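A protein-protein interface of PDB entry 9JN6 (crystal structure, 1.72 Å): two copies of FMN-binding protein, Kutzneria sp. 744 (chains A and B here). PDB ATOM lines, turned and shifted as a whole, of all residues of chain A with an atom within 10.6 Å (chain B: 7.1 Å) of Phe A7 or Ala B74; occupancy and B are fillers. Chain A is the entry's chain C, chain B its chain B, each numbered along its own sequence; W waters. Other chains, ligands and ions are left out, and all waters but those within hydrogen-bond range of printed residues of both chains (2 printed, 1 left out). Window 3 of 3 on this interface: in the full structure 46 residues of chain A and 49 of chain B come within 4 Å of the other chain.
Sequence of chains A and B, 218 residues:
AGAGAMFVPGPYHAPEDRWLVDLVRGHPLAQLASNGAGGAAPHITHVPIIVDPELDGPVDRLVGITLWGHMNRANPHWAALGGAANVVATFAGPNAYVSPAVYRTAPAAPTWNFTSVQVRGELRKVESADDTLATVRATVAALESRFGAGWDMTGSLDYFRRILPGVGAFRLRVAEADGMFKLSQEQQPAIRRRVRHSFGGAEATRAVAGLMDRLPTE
O of Ile B44 is in hydrogen-bond range of NE2 of Gln A118, at 3.0 Å.
ND2 of Asn B75 lies within hydrogen-bond range of OG1 of Thr B45 (3.2 Å). The side-chain sulfur (SD) of Met A6 lies close to the side-chain amide nitrogen (NE2) of Gln A118 (3.8 Å). OD1 of Asn B75 is in hydrogen-bond range of N of His B77 (2.9 Å). The backbone NH (N) of Arg A120 sits at hydrogen-bond distance from the backbone carbonyl oxygen (O) of Glu A176 (2.9 Å). The backbone NH of Gln A118 lies within hydrogen-bond range of the backbone carbonyl oxygen of Asp A178. The side-chain amide oxygen (OD1) of Asn B72 is in hydrogen-bond range of the backbone NH (N) of Ala B74 (2.9 Å).
Phe A7 touches Asn B72 (CE2 to ND2, 3.5 Å). O of Ala B74 touches CE1 of Phe A7, at 3.9 Å. Phe A7 touches Asn B75. Phe A7 touches Pro B76. Ile B44 touches Val A88 (CG1 to CG1, 3.7 Å). Ile B44 touches Thr A90 (CG2 to OG1, 3.99 Å). Arg A120 touches Ile B44.
Of chain B, only Asn B72 (3.5 Å), Ala B74 (3.9 Å), Asn B75 (3.4 Å) and Pro B76 (3.7 Å) come within 4 Å of Phe A7. Of the printed residues of chain B, Arg A120 touches Ile B44 (3.9 Å). Asn B72 touches one residue of chain A. Ala B74 touches just one residue of chain A: Phe A7. Of the printed residues of chain A, Asn B75 touches Phe A7 (3.4 Å). Of the printed residues of chain A, Pro B76 touches Phe A7. The nearest residue of chain A that does not touch Ala B74 is Pro A9 (7.7 Å). The nearest printed residue of chain B that does not touch Arg A120 is Thr B45 (6.9 Å).
Along chain B the printed residues that touch a printed residue of chain A span positions 44 to 76. Hydrophobic or aromatic side chains of chain A within 4 Å of the printed part of chain B: Phe A7 and Val A88. Among the printed residues, 8 pairs touch across the chains. Among the printed residues, no Asp or Glu carboxylate lies within 4 Å of a Lys or Arg side-chain nitrogen of the other chain.
No position is printed for both chains. Of the 8 pairs that touch across the chains among the printed residues, none has its exchanged pair printed and touching as well.
Water W1 lies within hydrogen-bond range of the backbone carbonyl oxygen (O) of Ala A5 (2.6 Å), the guanidinium group (NH2) of Arg A120 (2.9 Å), the backbone NH (N) of Ile B44 (3.0 Å) and the side-chain amide oxygen (OE1) of Gln A118 (3.3 Å). Water W2 lies within hydrogen-bond range of the backbone carbonyl oxygen of Ile B44 (2.7 Å), the side-chain hydroxyl of Thr B45 (3.2 Å) and the backbone NH of Phe A7 (3.3 Å).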
ATOM      1  N   ALA A   5      -9.199   0.679  -8.598  1.00  0.00           N
ATOM      2  CA  ALA A   5      -9.620   0.936  -7.176  1.00  0.00           C
ATOM      3  C   ALA A   5      -9.241   2.360  -6.741  1.00  0.00           C
ATOM      4  O   ALA A   5      -9.827   2.848  -5.762  1.00  0.00           O
ATOM      5  CB  ALA A   5      -9.019  -0.087  -6.245  1.00  0.00           C
ATOM      6  N   MET A   6      -8.265   2.985  -7.393  1.00  0.00           N
ATOM      7  CA  MET A   6      -8.014   4.437  -7.238  1.00  0.00           C
ATOM      8  C   MET A   6      -8.369   5.114  -8.559  1.00  0.00           C
ATOM      9  O   MET A   6      -7.902   4.658  -9.613  1.00  0.00           O
ATOM     10  CB  MET A   6      -6.545   4.703  -6.937  1.00  0.00           C
ATOM     11  CG  MET A   6      -6.238   6.130  -6.661  1.00  0.00           C
ATOM     12  SD  MET A   6      -4.447   6.311  -6.577  1.00  0.00           S
ATOM     13  CE  MET A   6      -4.400   8.056  -6.202  1.00  0.00           C
ATOM     14  N   PHE A   7      -9.105   6.218  -8.520  1.00  0.00           N
ATOM     15  CA  PHE A   7      -9.454   6.943  -9.768  1.00  0.00           C
ATOM     16  C   PHE A   7      -8.302   7.866 -10.158  1.00  0.00           C
ATOM     17  O   PHE A   7      -8.021   8.857  -9.424  1.00  0.00           O
ATOM     18  CB  PHE A   7     -10.733   7.757  -9.589  1.00  0.00           C
ATOM     19  CG  PHE A   7     -11.122   8.489 -10.838  1.00  0.00           C
ATOM     20  CD1 PHE A   7     -11.469   7.779 -11.976  1.00  0.00           C
ATOM     21  CD2 PHE A   7     -11.085   9.868 -10.892  1.00  0.00           C
ATOM     22  CE1 PHE A   7     -11.827   8.447 -13.143  1.00  0.00           C
ATOM     23  CE2 PHE A   7     -11.440  10.531 -12.056  1.00  0.00           C
ATOM     24  CZ  PHE A   7     -11.808   9.819 -13.177  1.00  0.00           C
ATOM     25  N   VAL A   8      -7.661   7.596 -11.287  1.00  0.00           N
ATOM     26  CA  VAL A   8      -6.582   8.480 -11.809  1.00  0.00           C
ATOM     27  C   VAL A   8      -6.937   8.865 -13.227  1.00  0.00           C
ATOM     28  O   VAL A   8      -6.941   7.991 -14.093  1.00  0.00           O
ATOM     29  CB  VAL A   8      -5.209   7.786 -11.765  1.00  0.00           C
ATOM     30  CG1 VAL A   8      -4.118   8.721 -12.236  1.00  0.00           C
ATOM     31  CG2 VAL A   8      -4.902   7.269 -10.358  1.00  0.00           C
ATOM     32  N   PRO A   9      -7.267  10.146 -13.482  1.00  0.00           N
ATOM     33  CA  PRO A   9      -7.464  10.615 -14.852  1.00  0.00           C
ATOM     34  C   PRO A   9      -6.231  10.343 -15.724  1.00  0.00           C
ATOM     35  O   PRO A   9      -5.109  10.451 -15.264  1.00  0.00           O
ATOM     36  CB  PRO A   9      -7.768  12.117 -14.704  1.00  0.00           C
ATOM     37  CG  PRO A   9      -8.207  12.282 -13.235  1.00  0.00           C
ATOM     38  CD  PRO A   9      -7.421  11.213 -12.493  1.00  0.00           C
ATOM     39  N   GLY A  10      -6.469   9.980 -16.990  1.00  0.00           N
ATOM     40  CA  GLY A  10      -5.418   9.584 -17.947  1.00  0.00           C
ATOM     41  C   GLY A  10      -4.172  10.464 -17.913  1.00  0.00           C
ATOM     42  O   GLY A  10      -3.058   9.925 -17.838  1.00  0.00           O
ATOM     43  N   PRO A  11      -4.297  11.823 -17.949  1.00  0.00           N
ATOM     44  CA  PRO A  11      -3.142  12.697 -18.043  1.00  0.00           C
ATOM     45  C   PRO A  11      -2.287  12.641 -16.771  1.00  0.00           C
ATOM     46  O   PRO A  11      -1.181  13.111 -16.849  1.00  0.00           O
ATOM     47  CB  PRO A  11      -3.700  14.117 -18.207  1.00  0.00           C
ATOM     48  CG  PRO A  11      -5.134  13.912 -18.570  1.00  0.00           C
ATOM     49  CD  PRO A  11      -5.545  12.604 -17.931  1.00  0.00           C
ATOM     50  N   TYR A  12      -2.791  12.052 -15.683  1.00  0.00           N
ATOM     51  CA  TYR A  12      -2.068  12.079 -14.383  1.00  0.00           C
ATOM     52  C   TYR A  12      -1.410  10.719 -14.110  1.00  0.00           C
ATOM     53  O   TYR A  12      -0.879  10.486 -12.978  1.00  0.00           O
ATOM     54  CB  TYR A  12      -3.003  12.523 -13.254  1.00  0.00           C
ATOM     55  CG  TYR A  12      -3.626  13.884 -13.448  1.00  0.00           C
ATOM     56  CD1 TYR A  12      -2.933  14.900 -14.084  1.00  0.00           C
ATOM     57  CD2 TYR A  12      -4.908  14.158 -13.014  1.00  0.00           C
ATOM     58  CE1 TYR A  12      -3.509  16.134 -14.285  1.00  0.00           C
ATOM     59  CE2 TYR A  12      -5.505  15.395 -13.202  1.00  0.00           C
ATOM     60  CZ  TYR A  12      -4.797  16.380 -13.868  1.00  0.00           C
ATOM     61  OH  TYR A  12      -5.303  17.633 -14.098  1.00  0.00           O
ATOM     62  N   HIS A  13      -1.353   9.835 -15.108  1.00  0.00           N
ATOM     63  CA  HIS A  13      -0.613   8.558 -14.943  1.00  0.00           C
ATOM     64  C   HIS A  13       0.880   8.833 -14.957  1.00  0.00           C
ATOM     65  O   HIS A  13       1.341   9.657 -15.745  1.00  0.00           O
ATOM     66  CB  HIS A  13      -1.032   7.539 -16.016  1.00  0.00           C
ATOM     67  CG  HIS A  13      -2.402   7.025 -15.779  1.00  0.00           C
ATOM     68  ND1 HIS A  13      -2.673   5.676 -15.634  1.00  0.00           N
ATOM     69  CD2 HIS A  13      -3.577   7.654 -15.571  1.00  0.00           C
ATOM     70  CE1 HIS A  13      -3.959   5.509 -15.372  1.00  0.00           C
ATOM     71  NE2 HIS A  13      -4.529   6.698 -15.340  1.00  0.00           N
ATOM     72  N   VAL A  88      -5.766  -0.605   2.146  1.00  0.00           N
ATOM     73  CA  VAL A  88      -5.066   0.346   1.250  1.00  0.00           C
ATOM     74  C   VAL A  88      -4.007   1.086   2.044  1.00  0.00           C
ATOM     75  O   VAL A  88      -4.265   1.457   3.218  1.00  0.00           O
ATOM     76  CB  VAL A  88      -6.024   1.315   0.534  1.00  0.00           C
ATOM     77  CG1 VAL A  88      -6.952   2.024   1.506  1.00  0.00           C
ATOM     78  CG2 VAL A  88      -5.246   2.317  -0.300  1.00  0.00           C
ATOM     79  N   THR A  90      -1.642   4.497   1.543  1.00  0.00           N
ATOM     80  CA  THR A  90      -1.531   5.705   0.710  1.00  0.00           C
ATOM     81  C   THR A  90      -0.244   6.435   1.087  1.00  0.00           C
ATOM     82  O   THR A  90       0.010   6.767   2.315  1.00  0.00           O
ATOM     83  CB  THR A  90      -2.743   6.625   0.812  1.00  0.00           C
ATOM     84  OG1 THR A  90      -3.891   5.840   0.495  1.00  0.00           O
ATOM     85  CG2 THR A  90      -2.587   7.820  -0.112  1.00  0.00           C
ATOM     86  N   PHE A 114      -0.423  17.418  -6.937  1.00  0.00           N
ATOM     87  CA  PHE A 114      -0.012  16.510  -5.869  1.00  0.00           C
ATOM     88  C   PHE A 114       0.335  15.166  -6.471  1.00  0.00           C
ATOM     89  O   PHE A 114      -0.013  14.834  -7.666  1.00  0.00           O
ATOM     90  CB  PHE A 114      -1.113  16.394  -4.824  1.00  0.00           C
ATOM     91  CG  PHE A 114      -2.298  15.577  -5.252  1.00  0.00           C
ATOM     92  CD1 PHE A 114      -3.375  16.153  -5.906  1.00  0.00           C
ATOM     93  CD2 PHE A 114      -2.388  14.237  -4.895  1.00  0.00           C
ATOM     94  CE1 PHE A 114      -4.498  15.391  -6.220  1.00  0.00           C
ATOM     95  CE2 PHE A 114      -3.469  13.463  -5.274  1.00  0.00           C
ATOM     96  CZ  PHE A 114      -4.536  14.045  -5.935  1.00  0.00           C
ATOM     97  N   THR A 115       1.004  14.396  -5.646  1.00  0.00           N
ATOM     98  CA  THR A 115       1.488  13.027  -5.972  1.00  0.00           C
ATOM     99  C   THR A 115       0.974  12.059  -4.926  1.00  0.00           C
ATOM    100  O   THR A 115       1.111  12.294  -3.730  1.00  0.00           O
ATOM    101  CB  THR A 115       3.003  13.056  -6.182  1.00  0.00           C
ATOM    102  OG1 THR A 115       3.599  13.554  -4.981  1.00  0.00           O
ATOM    103  CG2 THR A 115       3.335  13.863  -7.423  1.00  0.00           C
ATOM    104  N   SER A 116       0.398  10.957  -5.352  1.00  0.00           N
ATOM    105  CA  SER A 116      -0.093   9.916  -4.432  1.00  0.00           C
ATOM    106  C   SER A 116       0.202   8.562  -5.030  1.00  0.00           C
ATOM    107  O   SER A 116      -0.030   8.380  -6.203  1.00  0.00           O
ATOM    108  CB  SER A 116      -1.578  10.127  -4.202  1.00  0.00           C
ATOM    109  OG  SER A 116      -2.056   9.486  -3.049  1.00  0.00           O
ATOM    110  N   VAL A 117       0.550   7.597  -4.184  1.00  0.00           N
ATOM    111  CA  VAL A 117       0.473   6.168  -4.562  1.00  0.00           C
ATOM    112  C   VAL A 117      -0.487   5.487  -3.571  1.00  0.00           C
ATOM    113  O   VAL A 117      -0.272   5.590  -2.372  1.00  0.00           O
ATOM    114  CB  VAL A 117       1.853   5.508  -4.605  1.00  0.00           C
ATOM    115  CG1 VAL A 117       1.796   3.978  -4.697  1.00  0.00           C
ATOM    116  CG2 VAL A 117       2.654   6.055  -5.754  1.00  0.00           C
ATOM    117  N   GLN A 118      -1.440   4.746  -4.087  1.00  0.00           N
ATOM    118  CA  GLN A 118      -2.324   3.860  -3.323  1.00  0.00           C
ATOM    119  C   GLN A 118      -2.006   2.429  -3.675  1.00  0.00           C
ATOM    120  O   GLN A 118      -2.137   2.040  -4.866  1.00  0.00           O
ATOM    121  CB  GLN A 118      -3.799   4.136  -3.512  1.00  0.00           C
ATOM    122  CG  GLN A 118      -4.171   5.506  -3.043  1.00  0.00           C
ATOM    123  CD  GLN A 118      -5.637   5.776  -3.269  1.00  0.00           C
ATOM    124  OE1 GLN A 118      -6.440   4.873  -3.440  1.00  0.00           O
ATOM    125  NE2 GLN A 118      -5.990   7.037  -3.224  1.00  0.00           N
ATOM    126  N   VAL A 119      -1.547   1.692  -2.690  1.00  0.00           N
ATOM    127  CA  VAL A 119      -1.361   0.209  -2.839  1.00  0.00           C
ATOM    128  C   VAL A 119      -2.446  -0.545  -2.077  1.00  0.00           C
ATOM    129  O   VAL A 119      -2.871  -0.139  -0.959  1.00  0.00           O
ATOM    130  CB  VAL A 119       0.011  -0.322  -2.420  1.00  0.00           C
ATOM    131  CG1 VAL A 119       1.109   0.266  -3.260  1.00  0.00           C
ATOM    132  CG2 VAL A 119       0.267  -0.102  -0.960  1.00  0.00           C
ATOM    133  N   ARG A 120      -2.930  -1.599  -2.701  1.00  0.00           N
ATOM    134  CA  ARG A 120      -3.992  -2.414  -2.087  1.00  0.00           C
ATOM    135  C   ARG A 120      -3.578  -3.883  -2.103  1.00  0.00           C
ATOM    136  O   ARG A 120      -2.945  -4.372  -3.129  1.00  0.00           O
ATOM    137  CB  ARG A 120      -5.321  -2.221  -2.804  1.00  0.00           C
ATOM    138  CG  ARG A 120      -5.943  -0.849  -2.597  1.00  0.00           C
ATOM    139  CD  ARG A 120      -7.157  -0.662  -3.509  1.00  0.00           C
ATOM    140  NE  ARG A 120      -7.939   0.453  -3.012  1.00  0.00           N
ATOM    141  CZ  ARG A 120      -7.630   1.751  -3.142  1.00  0.00           C
ATOM    142  NH1 ARG A 120      -6.541   2.206  -3.759  1.00  0.00           N
ATOM    143  NH2 ARG A 120      -8.456   2.623  -2.596  1.00  0.00           N
ATOM    144  N   GLU A 176      -2.745  -4.539  -6.150  1.00  0.00           N
ATOM    145  CA  GLU A 176      -3.148  -3.387  -7.001  1.00  0.00           C
ATOM    146  C   GLU A 176      -2.267  -2.198  -6.619  1.00  0.00           C
ATOM    147  O   GLU A 176      -2.059  -1.969  -5.419  1.00  0.00           O
ATOM    148  CB  GLU A 176      -4.598  -2.954  -6.744  1.00  0.00           C
ATOM    149  CG  GLU A 176      -5.675  -3.712  -7.507  1.00  0.00           C
ATOM    150  CD  GLU A 176      -6.908  -2.837  -7.733  1.00  0.00           C
ATOM    151  OE1 GLU A 176      -7.981  -3.148  -7.150  1.00  0.00           O
ATOM    152  OE2 GLU A 176      -6.792  -1.813  -8.481  1.00  0.00           O
ATOM    153  N   ALA A 177      -1.792  -1.426  -7.568  1.00  0.00           N
ATOM    154  CA  ALA A 177      -1.052  -0.171  -7.258  1.00  0.00           C
ATOM    155  C   ALA A 177      -1.440   0.878  -8.273  1.00  0.00           C
ATOM    156  O   ALA A 177      -1.438   0.590  -9.501  1.00  0.00           O
ATOM    157  CB  ALA A 177       0.431  -0.383  -7.248  1.00  0.00           C
ATOM    158  N   ASP A 178      -1.789   2.056  -7.771  1.00  0.00           N
ATOM    159  CA  ASP A 178      -2.269   3.192  -8.582  1.00  0.00           C
ATOM    160  C   ASP A 178      -1.432   4.412  -8.178  1.00  0.00           C
ATOM    161  O   ASP A 178      -1.087   4.536  -6.982  1.00  0.00           O
ATOM    162  CB  ASP A 178      -3.781   3.350  -8.365  1.00  0.00           C
ATOM    163  CG  ASP A 178      -4.606   2.221  -8.989  1.00  0.00           C
ATOM    164  OD1 ASP A 178      -5.277   1.415  -8.213  1.00  0.00           O
ATOM    165  OD2 ASP A 178      -4.570   2.137 -10.255  1.00  0.00           O
ATOM    166  N   GLY A 179      -1.080   5.239  -9.146  1.00  0.00           N
ATOM    167  CA  GLY A 179      -0.301   6.468  -8.904  1.00  0.00           C
ATOM    168  C   GLY A 179      -0.925   7.692  -9.558  1.00  0.00           C
ATOM    169  O   GLY A 179      -1.187   7.665 -10.766  1.00  0.00           O
ATOM    170  N   MET A 180      -1.257   8.668  -8.751  1.00  0.00           N
ATOM    171  CA  MET A 180      -1.750   9.999  -9.148  1.00  0.00           C
ATOM    172  C   MET A 180      -0.531  10.905  -9.268  1.00  0.00           C
ATOM    173  O   MET A 180       0.105  11.243  -8.207  1.00  0.00           O
ATOM    174  CB  MET A 180      -2.729  10.564  -8.113  1.00  0.00           C
ATOM    175  CG  MET A 180      -3.199  11.954  -8.386  1.00  0.00           C
ATOM    176  SD  MET A 180      -4.480  12.067  -9.683  1.00  0.00           S
ATOM    177  CE  MET A 180      -5.844  11.381  -8.766  1.00  0.00           C
ATOM    178  N   PHE A 181      -0.202  11.339 -10.483  1.00  0.00           N
ATOM    179  CA  PHE A 181       0.854  12.357 -10.654  1.00  0.00           C
ATOM    180  C   PHE A 181       0.197  13.600 -11.277  1.00  0.00           C
ATOM    181  O   PHE A 181       0.219  13.788 -12.530  1.00  0.00           O
ATOM    182  CB  PHE A 181       2.034  11.769 -11.405  1.00  0.00           C
ATOM    183  CG  PHE A 181       2.746  10.726 -10.602  1.00  0.00           C
ATOM    184  CD1 PHE A 181       2.225   9.447 -10.482  1.00  0.00           C
ATOM    185  CD2 PHE A 181       3.876  11.058  -9.881  1.00  0.00           C
ATOM    186  CE1 PHE A 181       2.882   8.485  -9.732  1.00  0.00           C
ATOM    187  CE2 PHE A 181       4.536  10.087  -9.139  1.00  0.00           C
ATOM    188  CZ  PHE A 181       4.026   8.815  -9.057  1.00  0.00           C
ATOM    189  N   LYS A 182      -0.460  14.378 -10.412  1.00  0.00           N
ATOM    190  CA  LYS A 182      -1.301  15.496 -10.877  1.00  0.00           C
ATOM    191  C   LYS A 182      -0.385  16.700 -10.988  1.00  0.00           C
ATOM    192  O   LYS A 182      -0.035  17.351  -9.928  1.00  0.00           O
ATOM    193  CB  LYS A 182      -2.514  15.697  -9.989  1.00  0.00           C
ATOM    194  CG  LYS A 182      -3.302  16.945 -10.353  1.00  0.00           C
ATOM    195  CD  LYS A 182      -4.659  17.060  -9.727  1.00  0.00           C
ATOM    196  CE  LYS A 182      -5.180  18.479  -9.914  1.00  0.00           C
ATOM    197  NZ  LYS A 182      -5.593  18.739 -11.304  1.00  0.00           N
ATOM    198  N   ILE B  44     -10.168   5.880  -1.290  1.00  0.00           N
ATOM    199  CA  ILE B  44      -9.415   7.051  -0.788  1.00  0.00           C
ATOM    200  C   ILE B  44      -9.301   8.063  -1.923  1.00  0.00           C
ATOM    201  O   ILE B  44      -8.865   7.693  -3.030  1.00  0.00           O
ATOM    202  CB  ILE B  44      -8.006   6.655  -0.315  1.00  0.00           C
ATOM    203  CG1 ILE B  44      -7.982   5.466   0.652  1.00  0.00           C
ATOM    204  CG2 ILE B  44      -7.307   7.883   0.230  1.00  0.00           C
ATOM    205  CD1 ILE B  44      -8.137   5.923   2.075  1.00  0.00           C
ATOM    206  N   THR B  45      -9.771   9.294  -1.692  1.00  0.00           N
ATOM    207  CA  THR B  45      -9.644  10.384  -2.655  1.00  0.00           C
ATOM    208  C   THR B  45      -9.047  11.618  -1.997  1.00  0.00           C
ATOM    209  O   THR B  45      -9.527  11.969  -0.880  1.00  0.00           O
ATOM    210  CB  THR B  45     -11.003  10.716  -3.295  1.00  0.00           C
ATOM    211  OG1 THR B  45     -11.499   9.500  -3.874  1.00  0.00           O
ATOM    212  CG2 THR B  45     -10.796  11.759  -4.373  1.00  0.00           C
ATOM    213  N   MET B  71     -15.347  16.976  -5.169  1.00  0.00           N
ATOM    214  CA  MET B  71     -14.568  15.912  -5.809  1.00  0.00           C
ATOM    215  C   MET B  71     -15.179  15.783  -7.192  1.00  0.00           C
ATOM    216  O   MET B  71     -16.096  16.554  -7.499  1.00  0.00           O
ATOM    217  CB  MET B  71     -14.656  14.602  -5.018  1.00  0.00           C
ATOM    218  CG  MET B  71     -15.996  13.958  -5.029  1.00  0.00           C
ATOM    219  SD  MET B  71     -15.863  12.250  -4.366  1.00  0.00           S
ATOM    220  CE  MET B  71     -16.008  12.744  -2.686  1.00  0.00           C
ATOM    221  N   ASN B  72     -14.614  14.915  -7.986  1.00  0.00           N
ATOM    222  CA  ASN B  72     -15.075  14.644  -9.378  1.00  0.00           C
ATOM    223  C   ASN B  72     -16.259  13.666  -9.328  1.00  0.00           C
ATOM    224  O   ASN B  72     -16.068  12.543  -8.814  1.00  0.00           O
ATOM    225  CB  ASN B  72     -13.882  14.086 -10.124  1.00  0.00           C
ATOM    226  CG  ASN B  72     -14.147  13.874 -11.585  1.00  0.00           C
ATOM    227  OD1 ASN B  72     -15.253  14.081 -12.014  1.00  0.00           O
ATOM    228  ND2 ASN B  72     -13.087  13.630 -12.325  1.00  0.00           N
ATOM    229  N   ARG B  73     -17.405  14.019  -9.933  1.00  0.00           N
ATOM    230  CA  ARG B  73     -18.539  13.057 -10.081  1.00  0.00           C
ATOM    231  C   ARG B  73     -18.139  11.816 -10.873  1.00  0.00           C
ATOM    232  O   ARG B  73     -18.805  10.792 -10.658  1.00  0.00           O
ATOM    233  CB  ARG B  73     -19.742  13.731 -10.752  1.00  0.00           C
ATOM    234  CG  ARG B  73     -20.552  14.598  -9.801  1.00  0.00           C
ATOM    235  CD  ARG B  73     -21.640  15.427 -10.495  1.00  0.00           C
ATOM    236  NE  ARG B  73     -22.268  16.218  -9.470  1.00  0.00           N
ATOM    237  CZ  ARG B  73     -23.351  15.888  -8.794  1.00  0.00           C
ATOM    238  NH1 ARG B  73     -24.029  14.788  -9.112  1.00  0.00           N
ATOM    239  NH2 ARG B  73     -23.776  16.678  -7.812  1.00  0.00           N
ATOM    240  N   ALA B  74     -17.163  11.921 -11.774  1.00  0.00           N
ATOM    241  CA  ALA B  74     -16.674  10.837 -12.651  1.00  0.00           C
ATOM    242  C   ALA B  74     -15.892   9.811 -11.828  1.00  0.00           C
ATOM    243  O   ALA B  74     -15.655   8.718 -12.323  1.00  0.00           O
ATOM    244  CB  ALA B  74     -15.805  11.367 -13.747  1.00  0.00           C
ATOM    245  N   ASN B  75     -15.360  10.222 -10.674  1.00  0.00           N
ATOM    246  CA  ASN B  75     -14.620   9.343  -9.741  1.00  0.00           C
ATOM    247  C   ASN B  75     -15.611   8.327  -9.183  1.00  0.00           C
ATOM    248  O   ASN B  75     -16.557   8.717  -8.513  1.00  0.00           O
ATOM    249  CB  ASN B  75     -14.037  10.194  -8.597  1.00  0.00           C
ATOM    250  CG  ASN B  75     -13.189   9.404  -7.633  1.00  0.00           C
ATOM    251  OD1 ASN B  75     -13.322   8.181  -7.495  1.00  0.00           O
ATOM    252  ND2 ASN B  75     -12.363  10.119  -6.903  1.00  0.00           N
ATOM    253  N   PRO B  76     -15.395   6.992  -9.317  1.00  0.00           N
ATOM    254  CA  PRO B  76     -16.315   6.005  -8.730  1.00  0.00           C
ATOM    255  C   PRO B  76     -16.613   6.174  -7.242  1.00  0.00           C
ATOM    256  O   PRO B  76     -17.599   5.683  -6.683  1.00  0.00           O
ATOM    257  CB  PRO B  76     -15.566   4.691  -8.901  1.00  0.00           C
ATOM    258  CG  PRO B  76     -14.642   4.914 -10.078  1.00  0.00           C
ATOM    259  CD  PRO B  76     -14.263   6.388 -10.031  1.00  0.00           C
ATOM    260  N   HIS B  77     -15.728   6.868  -6.555  1.00  0.00           N
ATOM    261  CA  HIS B  77     -15.887   7.102  -5.113  1.00  0.00           C
ATOM    262  C   HIS B  77     -17.170   7.921  -4.875  1.00  0.00           C
ATOM    263  O   HIS B  77     -17.894   7.669  -3.879  1.00  0.00           O
ATOM    264  CB  HIS B  77     -14.611   7.778  -4.609  1.00  0.00           C
ATOM    265  CG  HIS B  77     -14.536   7.840  -3.134  1.00  0.00           C
ATOM    266  ND1 HIS B  77     -13.440   8.397  -2.466  1.00  0.00           N
ATOM    267  CD2 HIS B  77     -15.364   7.377  -2.185  1.00  0.00           C
ATOM    268  CE1 HIS B  77     -13.632   8.272  -1.175  1.00  0.00           C
ATOM    269  NE2 HIS B  77     -14.771   7.623  -0.985  1.00  0.00           N
ATOM    270  N   TRP B  78     -17.437   8.884  -5.742  1.00  0.00           N
ATOM    271  CA  TRP B  78     -18.685   9.696  -5.641  1.00  0.00           C
ATOM    272  C   TRP B  78     -19.927   8.778  -5.597  1.00  0.00           C
ATOM    273  O   TRP B  78     -20.734   8.888  -4.686  1.00  0.00           O
ATOM    274  CB  TRP B  78     -18.715  10.700  -6.788  1.00  0.00           C
ATOM    275  CG  TRP B  78     -19.955  11.521  -6.837  1.00  0.00           C
ATOM    276  CD1 TRP B  78     -21.006  11.357  -7.694  1.00  0.00           C
ATOM    277  CD2 TRP B  78     -20.296  12.621  -5.968  1.00  0.00           C
ATOM    278  NE1 TRP B  78     -21.980  12.280  -7.416  1.00  0.00           N
ATOM    279  CE2 TRP B  78     -21.581  13.060  -6.363  1.00  0.00           C
ATOM    280  CE3 TRP B  78     -19.666  13.268  -4.886  1.00  0.00           C
ATOM    281  CZ2 TRP B  78     -22.190  14.157  -5.769  1.00  0.00           C
ATOM    282  CZ3 TRP B  78     -20.284  14.335  -4.280  1.00  0.00           C
ATOM    283  CH2 TRP B  78     -21.532  14.778  -4.723  1.00  0.00           C
ATOM    284  N   ALA B  79     -20.141   7.920  -6.595  1.00  0.00           N
ATOM    285  CA  ALA B  79     -21.284   6.971  -6.580  1.00  0.00           C
ATOM    286  C   ALA B  79     -21.232   6.081  -5.330  1.00  0.00           C
ATOM    287  O   ALA B  79     -22.279   5.795  -4.755  1.00  0.00           O
ATOM    288  CB  ALA B  79     -21.283   6.141  -7.853  1.00  0.00           C
ATOM    289  N   GLY B 166     -19.358  18.554 -13.533  1.00  0.00           N
ATOM    290  CA  GLY B 166     -18.453  17.497 -13.109  1.00  0.00           C
ATOM    291  C   GLY B 166     -18.163  17.622 -11.624  1.00  0.00           C
ATOM    292  O   GLY B 166     -17.742  16.647 -11.023  1.00  0.00           O
ATOM    293  N   VAL B 167     -18.489  18.773 -11.031  1.00  0.00           N
ATOM    294  CA  VAL B 167     -18.272  18.948  -9.558  1.00  0.00           C
ATOM    295  C   VAL B 167     -19.266  18.129  -8.728  1.00  0.00           C
ATOM    296  O   VAL B 167     -20.491  18.348  -8.849  1.00  0.00           O
ATOM    297  CB  VAL B 167     -18.364  20.426  -9.181  1.00  0.00           C
ATOM    298  CG1 VAL B 167     -18.107  20.599  -7.680  1.00  0.00           C
ATOM    299  CG2 VAL B 167     -17.409  21.224 -10.024  1.00  0.00           C
ATOM    300  N   GLY B 168     -18.747  17.340  -7.781  1.00  0.00           N
ATOM    301  CA  GLY B 168     -19.505  16.670  -6.718  1.00  0.00           C
ATOM    302  C   GLY B 168     -19.233  17.332  -5.396  1.00  0.00           C
ATOM    303  O   GLY B 168     -18.218  17.024  -4.739  1.00  0.00           O
HETATM  304  O   HOH W   1      -9.708   4.855  -4.051  1.00  0.00           O
HETATM  305  O   HOH W   2      -9.641   7.550  -5.586  1.00  0.00           O
